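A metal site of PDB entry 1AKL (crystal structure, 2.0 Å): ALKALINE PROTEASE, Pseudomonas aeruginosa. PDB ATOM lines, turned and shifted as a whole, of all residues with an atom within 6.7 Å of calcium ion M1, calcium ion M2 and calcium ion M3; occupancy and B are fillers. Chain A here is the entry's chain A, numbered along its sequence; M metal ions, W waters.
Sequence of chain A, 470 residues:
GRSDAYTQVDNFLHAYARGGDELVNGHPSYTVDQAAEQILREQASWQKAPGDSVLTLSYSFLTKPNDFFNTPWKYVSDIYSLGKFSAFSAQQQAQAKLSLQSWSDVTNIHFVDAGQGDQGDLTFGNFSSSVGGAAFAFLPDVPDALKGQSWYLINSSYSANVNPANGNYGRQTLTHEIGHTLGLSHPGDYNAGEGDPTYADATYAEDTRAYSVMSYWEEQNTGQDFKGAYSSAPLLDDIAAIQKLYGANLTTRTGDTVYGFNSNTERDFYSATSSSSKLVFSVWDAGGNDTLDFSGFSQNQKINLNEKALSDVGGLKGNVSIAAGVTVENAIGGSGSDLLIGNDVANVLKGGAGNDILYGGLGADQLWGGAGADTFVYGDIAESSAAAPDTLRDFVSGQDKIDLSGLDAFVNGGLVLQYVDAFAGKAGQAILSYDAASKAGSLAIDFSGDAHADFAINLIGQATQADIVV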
ATOM      1  N   GLN A 299       7.221  13.859  10.326  1.00  0.00           N
ATOM      2  CA  GLN A 299       6.114  14.719   9.928  1.00  0.00           C
ATOM      3  C   GLN A 299       6.298  15.281   8.537  1.00  0.00           C
ATOM      4  O   GLN A 299       7.405  15.284   7.998  1.00  0.00           O
ATOM      5  CB  GLN A 299       5.979  15.891  10.893  1.00  0.00           C
ATOM      6  CG  GLN A 299       5.667  15.510  12.298  1.00  0.00           C
ATOM      7  CD  GLN A 299       6.888  15.274  13.111  1.00  0.00           C
ATOM      8  OE1 GLN A 299       7.972  15.053  12.587  1.00  0.00           O
ATOM      9  NE2 GLN A 299       6.729  15.327  14.416  1.00  0.00           N
ATOM     10  N   GLN A 301       6.963  18.064   6.188  1.00  0.00           N
ATOM     11  CA  GLN A 301       7.660  19.327   6.377  1.00  0.00           C
ATOM     12  C   GLN A 301       7.717  20.170   5.116  1.00  0.00           C
ATOM     13  O   GLN A 301       7.555  19.647   4.021  1.00  0.00           O
ATOM     14  CB  GLN A 301       9.088  19.028   6.831  1.00  0.00           C
ATOM     15  CG  GLN A 301       9.168  17.984   7.917  1.00  0.00           C
ATOM     16  CD  GLN A 301      10.595  17.740   8.353  1.00  0.00           C
ATOM     17  OE1 GLN A 301      11.154  18.535   9.119  1.00  0.00           O
ATOM     18  NE2 GLN A 301      11.196  16.676   7.877  1.00  0.00           N
ATOM     19  N   GLY A 333      15.075  16.280   3.589  1.00  0.00           N
ATOM     20  CA  GLY A 333      13.786  16.074   4.205  1.00  0.00           C
ATOM     21  C   GLY A 333      13.765  14.768   4.963  1.00  0.00           C
ATOM     22  O   GLY A 333      14.748  14.025   4.942  1.00  0.00           O
ATOM     23  N   GLY A 334      12.651  14.472   5.616  1.00  0.00           N
ATOM     24  CA  GLY A 334      12.518  13.237   6.372  1.00  0.00           C
ATOM     25  C   GLY A 334      11.625  12.233   5.669  1.00  0.00           C
ATOM     26  O   GLY A 334      11.319  12.383   4.494  1.00  0.00           O
ATOM     27  N   SER A 335      11.128  11.245   6.404  1.00  0.00           N
ATOM     28  CA  SER A 335      10.280  10.226   5.805  1.00  0.00           C
ATOM     29  C   SER A 335       8.853  10.654   5.480  1.00  0.00           C
ATOM     30  O   SER A 335       8.091   9.895   4.882  1.00  0.00           O
ATOM     31  CB  SER A 335      10.290   8.964   6.669  1.00  0.00           C
ATOM     32  OG  SER A 335       9.896   9.242   7.994  1.00  0.00           O
ATOM     33  N   GLY A 336       8.489  11.881   5.855  1.00  0.00           N
ATOM     34  CA  GLY A 336       7.152  12.356   5.556  1.00  0.00           C
ATOM     35  C   GLY A 336       7.153  12.918   4.145  1.00  0.00           C
ATOM     36  O   GLY A 336       8.214  12.997   3.503  1.00  0.00           O
ATOM     37  N   SER A 337       5.983  13.274   3.648  1.00  0.00           N
ATOM     38  CA  SER A 337       5.876  13.852   2.316  1.00  0.00           C
ATOM     39  C   SER A 337       6.189  15.333   2.460  1.00  0.00           C
ATOM     40  O   SER A 337       5.394  16.100   2.999  1.00  0.00           O
ATOM     41  CB  SER A 337       4.481  13.617   1.739  1.00  0.00           C
ATOM     42  OG  SER A 337       4.270  12.227   1.493  1.00  0.00           O
ATOM     43  N   ASP A 338       7.368  15.729   1.983  1.00  0.00           N
ATOM     44  CA  ASP A 338       7.857  17.097   2.118  1.00  0.00           C
ATOM     45  C   ASP A 338       7.782  17.967   0.876  1.00  0.00           C
ATOM     46  O   ASP A 338       7.603  17.485  -0.244  1.00  0.00           O
ATOM     47  CB  ASP A 338       9.307  17.076   2.581  1.00  0.00           C
ATOM     48  CG  ASP A 338       9.548  16.110   3.712  1.00  0.00           C
ATOM     49  OD1 ASP A 338       8.702  16.027   4.630  1.00  0.00           O
ATOM     50  OD2 ASP A 338      10.585  15.413   3.671  1.00  0.00           O
ATOM     51  N   LEU A 340      10.326  20.793  -0.691  1.00  0.00           N
ATOM     52  CA  LEU A 340      11.620  21.427  -0.557  1.00  0.00           C
ATOM     53  C   LEU A 340      11.849  22.435  -1.642  1.00  0.00           C
ATOM     54  O   LEU A 340      11.925  22.072  -2.805  1.00  0.00           O
ATOM     55  CB  LEU A 340      12.738  20.390  -0.598  1.00  0.00           C
ATOM     56  CG  LEU A 340      12.913  19.369   0.534  1.00  0.00           C
ATOM     57  CD1 LEU A 340      11.987  18.198   0.333  1.00  0.00           C
ATOM     58  CD2 LEU A 340      14.348  18.881   0.542  1.00  0.00           C
ATOM     59  N   LYS A 350      17.235  16.704  -1.011  1.00  0.00           N
ATOM     60  CA  LYS A 350      16.973  15.283  -0.884  1.00  0.00           C
ATOM     61  C   LYS A 350      15.655  15.094  -0.171  1.00  0.00           C
ATOM     62  O   LYS A 350      15.524  15.443   0.991  1.00  0.00           O
ATOM     63  CB  LYS A 350      18.095  14.588  -0.126  1.00  0.00           C
ATOM     64  CG  LYS A 350      19.429  14.633  -0.845  1.00  0.00           C
ATOM     65  CD  LYS A 350      20.470  13.825  -0.113  1.00  0.00           C
ATOM     66  CE  LYS A 350      21.743  13.691  -0.929  1.00  0.00           C
ATOM     67  NZ  LYS A 350      22.828  12.997  -0.165  1.00  0.00           N
ATOM     68  N   GLY A 351      14.675  14.536  -0.855  1.00  0.00           N
ATOM     69  CA  GLY A 351      13.383  14.366  -0.240  1.00  0.00           C
ATOM     70  C   GLY A 351      13.238  13.214   0.721  1.00  0.00           C
ATOM     71  O   GLY A 351      12.272  13.181   1.495  1.00  0.00           O
ATOM     72  N   GLY A 352      14.149  12.247   0.636  1.00  0.00           N
ATOM     73  CA  GLY A 352      14.073  11.090   1.510  1.00  0.00           C
ATOM     74  C   GLY A 352      12.815  10.303   1.196  1.00  0.00           C
ATOM     75  O   GLY A 352      12.222  10.480   0.130  1.00  0.00           O
ATOM     76  N   ALA A 353      12.366   9.452   2.114  1.00  0.00           N
ATOM     77  CA  ALA A 353      11.163   8.675   1.877  1.00  0.00           C
ATOM     78  C   ALA A 353       9.948   9.594   1.734  1.00  0.00           C
ATOM     79  O   ALA A 353      10.080  10.815   1.878  1.00  0.00           O
ATOM     80  CB  ALA A 353      10.939   7.671   2.993  1.00  0.00           C
ATOM     81  N   GLY A 354       8.793   9.027   1.445  1.00  0.00           N
ATOM     82  CA  GLY A 354       7.609   9.832   1.258  1.00  0.00           C
ATOM     83  C   GLY A 354       7.574  10.474  -0.118  1.00  0.00           C
ATOM     84  O   GLY A 354       8.602  10.570  -0.822  1.00  0.00           O
ATOM     85  N   ASN A 355       6.394  10.966  -0.481  1.00  0.00           N
ATOM     86  CA  ASN A 355       6.192  11.601  -1.777  1.00  0.00           C
ATOM     87  C   ASN A 355       6.437  13.097  -1.698  1.00  0.00           C
ATOM     88  O   ASN A 355       5.577  13.870  -1.294  1.00  0.00           O
ATOM     89  CB  ASN A 355       4.774  11.304  -2.273  1.00  0.00           C
ATOM     90  CG  ASN A 355       4.545   9.812  -2.489  1.00  0.00           C
ATOM     91  OD1 ASN A 355       5.497   9.025  -2.574  1.00  0.00           O
ATOM     92  ND2 ASN A 355       3.284   9.413  -2.568  1.00  0.00           N
ATOM     93  N   ASP A 356       7.620  13.500  -2.134  1.00  0.00           N
ATOM     94  CA  ASP A 356       8.055  14.886  -2.063  1.00  0.00           C
ATOM     95  C   ASP A 356       7.894  15.696  -3.327  1.00  0.00           C
ATOM     96  O   ASP A 356       7.822  15.162  -4.430  1.00  0.00           O
ATOM     97  CB  ASP A 356       9.517  14.934  -1.632  1.00  0.00           C
ATOM     98  CG  ASP A 356       9.828  13.953  -0.531  1.00  0.00           C
ATOM     99  OD1 ASP A 356       9.327  14.127   0.595  1.00  0.00           O
ATOM    100  OD2 ASP A 356      10.572  12.998  -0.794  1.00  0.00           O
ATOM    101  N   LEU A 358       9.951  18.641  -5.108  1.00  0.00           N
ATOM    102  CA  LEU A 358      11.231  19.340  -5.133  1.00  0.00           C
ATOM    103  C   LEU A 358      11.207  20.474  -6.158  1.00  0.00           C
ATOM    104  O   LEU A 358      10.848  20.266  -7.310  1.00  0.00           O
ATOM    105  CB  LEU A 358      12.367  18.376  -5.512  1.00  0.00           C
ATOM    106  CG  LEU A 358      12.733  17.098  -4.733  1.00  0.00           C
ATOM    107  CD1 LEU A 358      13.549  17.431  -3.531  1.00  0.00           C
ATOM    108  CD2 LEU A 358      11.525  16.264  -4.394  1.00  0.00           C
ATOM    109  N   TRP A 368      17.330  14.919  -5.580  1.00  0.00           N
ATOM    110  CA  TRP A 368      17.179  13.505  -5.243  1.00  0.00           C
ATOM    111  C   TRP A 368      15.805  13.369  -4.605  1.00  0.00           C
ATOM    112  O   TRP A 368      15.539  13.940  -3.570  1.00  0.00           O
ATOM    113  CB  TRP A 368      18.223  13.057  -4.224  1.00  0.00           C
ATOM    114  CG  TRP A 368      19.653  13.237  -4.596  1.00  0.00           C
ATOM    115  CD1 TRP A 368      20.333  14.426  -4.701  1.00  0.00           C
ATOM    116  CD2 TRP A 368      20.600  12.204  -4.856  1.00  0.00           C
ATOM    117  NE1 TRP A 368      21.660  14.181  -5.002  1.00  0.00           N
ATOM    118  CE2 TRP A 368      21.845  12.833  -5.105  1.00  0.00           C
ATOM    119  CE3 TRP A 368      20.519  10.806  -4.908  1.00  0.00           C
ATOM    120  CZ2 TRP A 368      22.997  12.108  -5.400  1.00  0.00           C
ATOM    121  CZ3 TRP A 368      21.671  10.081  -5.202  1.00  0.00           C
ATOM    122  CH2 TRP A 368      22.899  10.747  -5.443  1.00  0.00           C
ATOM    123  N   GLY A 369      14.925  12.587  -5.208  1.00  0.00           N
ATOM    124  CA  GLY A 369      13.615  12.433  -4.621  1.00  0.00           C
ATOM    125  C   GLY A 369      13.559  11.327  -3.592  1.00  0.00           C
ATOM    126  O   GLY A 369      12.673  11.316  -2.722  1.00  0.00           O
ATOM    127  N   GLY A 370      14.461  10.369  -3.712  1.00  0.00           N
ATOM    128  CA  GLY A 370      14.471   9.240  -2.796  1.00  0.00           C
ATOM    129  C   GLY A 370      13.273   8.330  -3.023  1.00  0.00           C
ATOM    130  O   GLY A 370      12.557   8.443  -4.028  1.00  0.00           O
ATOM    131  N   ALA A 371      13.029   7.445  -2.062  1.00  0.00           N
ATOM    132  CA  ALA A 371      11.914   6.511  -2.125  1.00  0.00           C
ATOM    133  C   ALA A 371      10.616   7.280  -2.355  1.00  0.00           C
ATOM    134  O   ALA A 371      10.552   8.488  -2.080  1.00  0.00           O
ATOM    135  CB  ALA A 371      11.834   5.727  -0.832  1.00  0.00           C
ATOM    136  N   GLY A 372       9.603   6.610  -2.892  1.00  0.00           N
ATOM    137  CA  GLY A 372       8.317   7.248  -3.132  1.00  0.00           C
ATOM    138  C   GLY A 372       8.185   7.978  -4.451  1.00  0.00           C
ATOM    139  O   GLY A 372       9.197   8.245  -5.137  1.00  0.00           O
ATOM    140  N   ALA A 373       6.959   8.337  -4.787  1.00  0.00           N
ATOM    141  CA  ALA A 373       6.634   9.042  -6.013  1.00  0.00           C
ATOM    142  C   ALA A 373       6.827  10.527  -5.767  1.00  0.00           C
ATOM    143  O   ALA A 373       5.997  11.167  -5.149  1.00  0.00           O
ATOM    144  CB  ALA A 373       5.201   8.769  -6.402  1.00  0.00           C
ATOM    145  N   ASP A 374       7.913  11.062  -6.308  1.00  0.00           N
ATOM    146  CA  ASP A 374       8.238  12.465  -6.106  1.00  0.00           C
ATOM    147  C   ASP A 374       8.017  13.280  -7.356  1.00  0.00           C
ATOM    148  O   ASP A 374       8.135  12.748  -8.461  1.00  0.00           O
ATOM    149  CB  ASP A 374       9.704  12.583  -5.675  1.00  0.00           C
ATOM    150  CG  ASP A 374      10.038  11.625  -4.568  1.00  0.00           C
ATOM    151  OD1 ASP A 374       9.416  11.707  -3.489  1.00  0.00           O
ATOM    152  OD2 ASP A 374      10.886  10.745  -4.803  1.00  0.00           O
ATOM    153  N   PHE A 376       9.117  16.786  -9.488  1.00  0.00           N
ATOM    154  CA  PHE A 376      10.162  17.784  -9.632  1.00  0.00           C
ATOM    155  C   PHE A 376       9.541  18.944 -10.411  1.00  0.00           C
ATOM    156  O   PHE A 376       9.321  18.852 -11.616  1.00  0.00           O
ATOM    157  CB  PHE A 376      11.371  17.183 -10.349  1.00  0.00           C
ATOM    158  CG  PHE A 376      11.903  15.927  -9.697  1.00  0.00           C
ATOM    159  CD1 PHE A 376      11.370  14.686 -10.013  1.00  0.00           C
ATOM    160  CD2 PHE A 376      12.894  15.997  -8.720  1.00  0.00           C
ATOM    161  CE1 PHE A 376      11.818  13.528  -9.369  1.00  0.00           C
ATOM    162  CE2 PHE A 376      13.337  14.856  -8.071  1.00  0.00           C
ATOM    163  CZ  PHE A 376      12.797  13.616  -8.399  1.00  0.00           C
ATOM    164  N   ASP A 394      18.194  10.508  -9.407  1.00  0.00           N
ATOM    165  CA  ASP A 394      17.582   9.211  -9.082  1.00  0.00           C
ATOM    166  C   ASP A 394      16.152   9.074  -9.598  1.00  0.00           C
ATOM    167  O   ASP A 394      15.247   8.617  -8.873  1.00  0.00           O
ATOM    168  CB  ASP A 394      17.621   8.988  -7.564  1.00  0.00           C
ATOM    169  CG  ASP A 394      16.722   9.938  -6.798  1.00  0.00           C
ATOM    170  OD1 ASP A 394      16.209  10.921  -7.384  1.00  0.00           O
ATOM    171  OD2 ASP A 394      16.515   9.680  -5.600  1.00  0.00           O
ATOM    172  N   PHE A 395      15.960   9.469 -10.860  1.00  0.00           N
ATOM    173  CA  PHE A 395      14.641   9.420 -11.467  1.00  0.00           C
ATOM    174  C   PHE A 395      14.179   7.985 -11.704  1.00  0.00           C
ATOM    175  O   PHE A 395      14.967   7.087 -12.013  1.00  0.00           O
ATOM    176  CB  PHE A 395      14.638  10.217 -12.773  1.00  0.00           C
ATOM    177  CG  PHE A 395      13.270  10.625 -13.222  1.00  0.00           C
ATOM    178  CD1 PHE A 395      12.674  11.779 -12.711  1.00  0.00           C
ATOM    179  CD2 PHE A 395      12.555   9.854 -14.139  1.00  0.00           C
ATOM    180  CE1 PHE A 395      11.391  12.166 -13.125  1.00  0.00           C
ATOM    181  CE2 PHE A 395      11.275  10.228 -14.548  1.00  0.00           C
ATOM    182  CZ  PHE A 395      10.694  11.383 -14.046  1.00  0.00           C
ATOM    183  N   VAL A 396      12.884   7.779 -11.531  1.00  0.00           N
ATOM    184  CA  VAL A 396      12.277   6.474 -11.708  1.00  0.00           C
ATOM    185  C   VAL A 396      11.022   6.649 -12.515  1.00  0.00           C
ATOM    186  O   VAL A 396       9.980   7.070 -11.998  1.00  0.00           O
ATOM    187  CB  VAL A 396      11.919   5.857 -10.349  1.00  0.00           C
ATOM    188  CG1 VAL A 396      10.963   4.685 -10.531  1.00  0.00           C
ATOM    189  CG2 VAL A 396      13.182   5.407  -9.654  1.00  0.00           C
ATOM    190  N   GLN A 399       7.021   6.484 -11.730  1.00  0.00           N
ATOM    191  CA  GLN A 399       6.898   6.726 -10.302  1.00  0.00           C
ATOM    192  C   GLN A 399       7.088   8.225 -10.060  1.00  0.00           C
ATOM    193  O   GLN A 399       6.249   8.869  -9.444  1.00  0.00           O
ATOM    194  CB  GLN A 399       7.938   5.920  -9.517  1.00  0.00           C
ATOM    195  CG  GLN A 399       7.674   5.883  -8.016  1.00  0.00           C
ATOM    196  CD  GLN A 399       8.846   5.301  -7.215  1.00  0.00           C
ATOM    197  OE1 GLN A 399       9.870   5.980  -6.996  1.00  0.00           O
ATOM    198  NE2 GLN A 399       8.687   4.072  -6.737  1.00  0.00           N
ATOM    199  N   ASP A 400       8.184   8.772 -10.572  1.00  0.00           N
ATOM    200  CA  ASP A 400       8.485  10.188 -10.430  1.00  0.00           C
ATOM    201  C   ASP A 400       7.931  10.959 -11.627  1.00  0.00           C
ATOM    202  O   ASP A 400       7.785  10.402 -12.720  1.00  0.00           O
ATOM    203  CB  ASP A 400      10.005  10.410 -10.363  1.00  0.00           C
ATOM    204  CG  ASP A 400      10.661   9.672  -9.209  1.00  0.00           C
ATOM    205  OD1 ASP A 400       9.965   9.180  -8.293  1.00  0.00           O
ATOM    206  OD2 ASP A 400      11.905   9.610  -9.229  1.00  0.00           O
HETATM  207 CA    CA M   1      10.816  10.730  -1.718  1.00  0.00          CA
HETATM  208 CA    CA M   2      10.275  12.983   2.636  1.00  0.00          CA
HETATM  209 CA    CA M   3      11.215   8.321  -6.089  1.00  0.00          CA
HETATM  210  O   HOH W   1      12.992   9.706  -6.901  1.00  0.00           O
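Calcium ion M3 is bound by O of Gly 372 (2.2 Å), water W1 (2.4 Å), O of Gly 370 (2.5 Å), OD1 of Asp 400 (2.7 Å), OD2 of Asp 374 (2.8 Å) and OE1 of Gln 399 (2.8 Å).
Residues that only touch calcium ion M2: Ser 335. Of the 30 residues printed, 8 come within 4 Å of calcium ion M2.
The side-chain carboxylate of Asp 394 is in hydrogen-bond range of the backbone NH of Gly 369 (3.0 Å). The side-chain amide nitrogen of Gln 301 sits close to the backbone NH of Gly 334, at 3.5 Å. N of Gly 351 sits at hydrogen-bond distance from O of Trp 368. The backbone NH (N) of Gly 370 is in hydrogen-bond range of the side-chain carboxylate (OD2) of Asp 394 (2.9 Å). The backbone NH (N) of Gln 301 is in hydrogen-bond range of the side-chain carboxylate (OD1) of Asp 338. OD2 of Asp 400 lies within hydrogen-bond range of N of Val 396.
Water W1 bridges OD2 of Asp 400 (2.6 Å) and O of Asp 394 (3.2 Å).
Within 4 Å of calcium ion M3: Gly 370, Ala 371, Gly 372, Asp 374, Gln 399 and Asp 400. The nearest printed residue that does not touch calcium ion M3 is Ala 373 (4.5 Å).
Within 4 Å of calcium ion M1: Gly 352, Ala 353, Gly 354, Asp 356, Gly 369, Gly 370, Ala 371 and Asp 374. Along chain A the residues within 4 Å of calcium ion M1 span positions 352 to 374.
Calcium ion M1 is bound by the backbone carbonyl oxygen of Gly 369 (2.2 Å), the backbone carbonyl oxygen of Ala 371 (2.3 Å), the backbone carbonyl oxygen of Gly 352 (2.3 Å), the backbone carbonyl oxygen of Gly 354 (2.4 Å), the side-chain carboxylate of Asp 374 (2.5 Å) and the side-chain carboxylate of Asp 356 (2.5 Å). Slightly farther from calcium ion M1 lies the side-chain carboxylate (OD2) of Asp 374 (3.1 Å).
Calcium ion M2 is bound by O of Gly 334 (2.2 Å). O of Gly 336 binds calcium ion M2. Calcium ion M2 is bound by the backbone carbonyl oxygen (O) of Ala 353. O of Gly 351 binds calcium ion M2 (2.3 Å). The side-chain carboxylate (OD1) of Asp 356 is bound to calcium ion M2 (2.5 Å). The side-chain carboxylate (OD2) of Asp 338 binds calcium ion M2 (2.7 Å). Calcium ion M2 has six donor atoms within binding distance.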
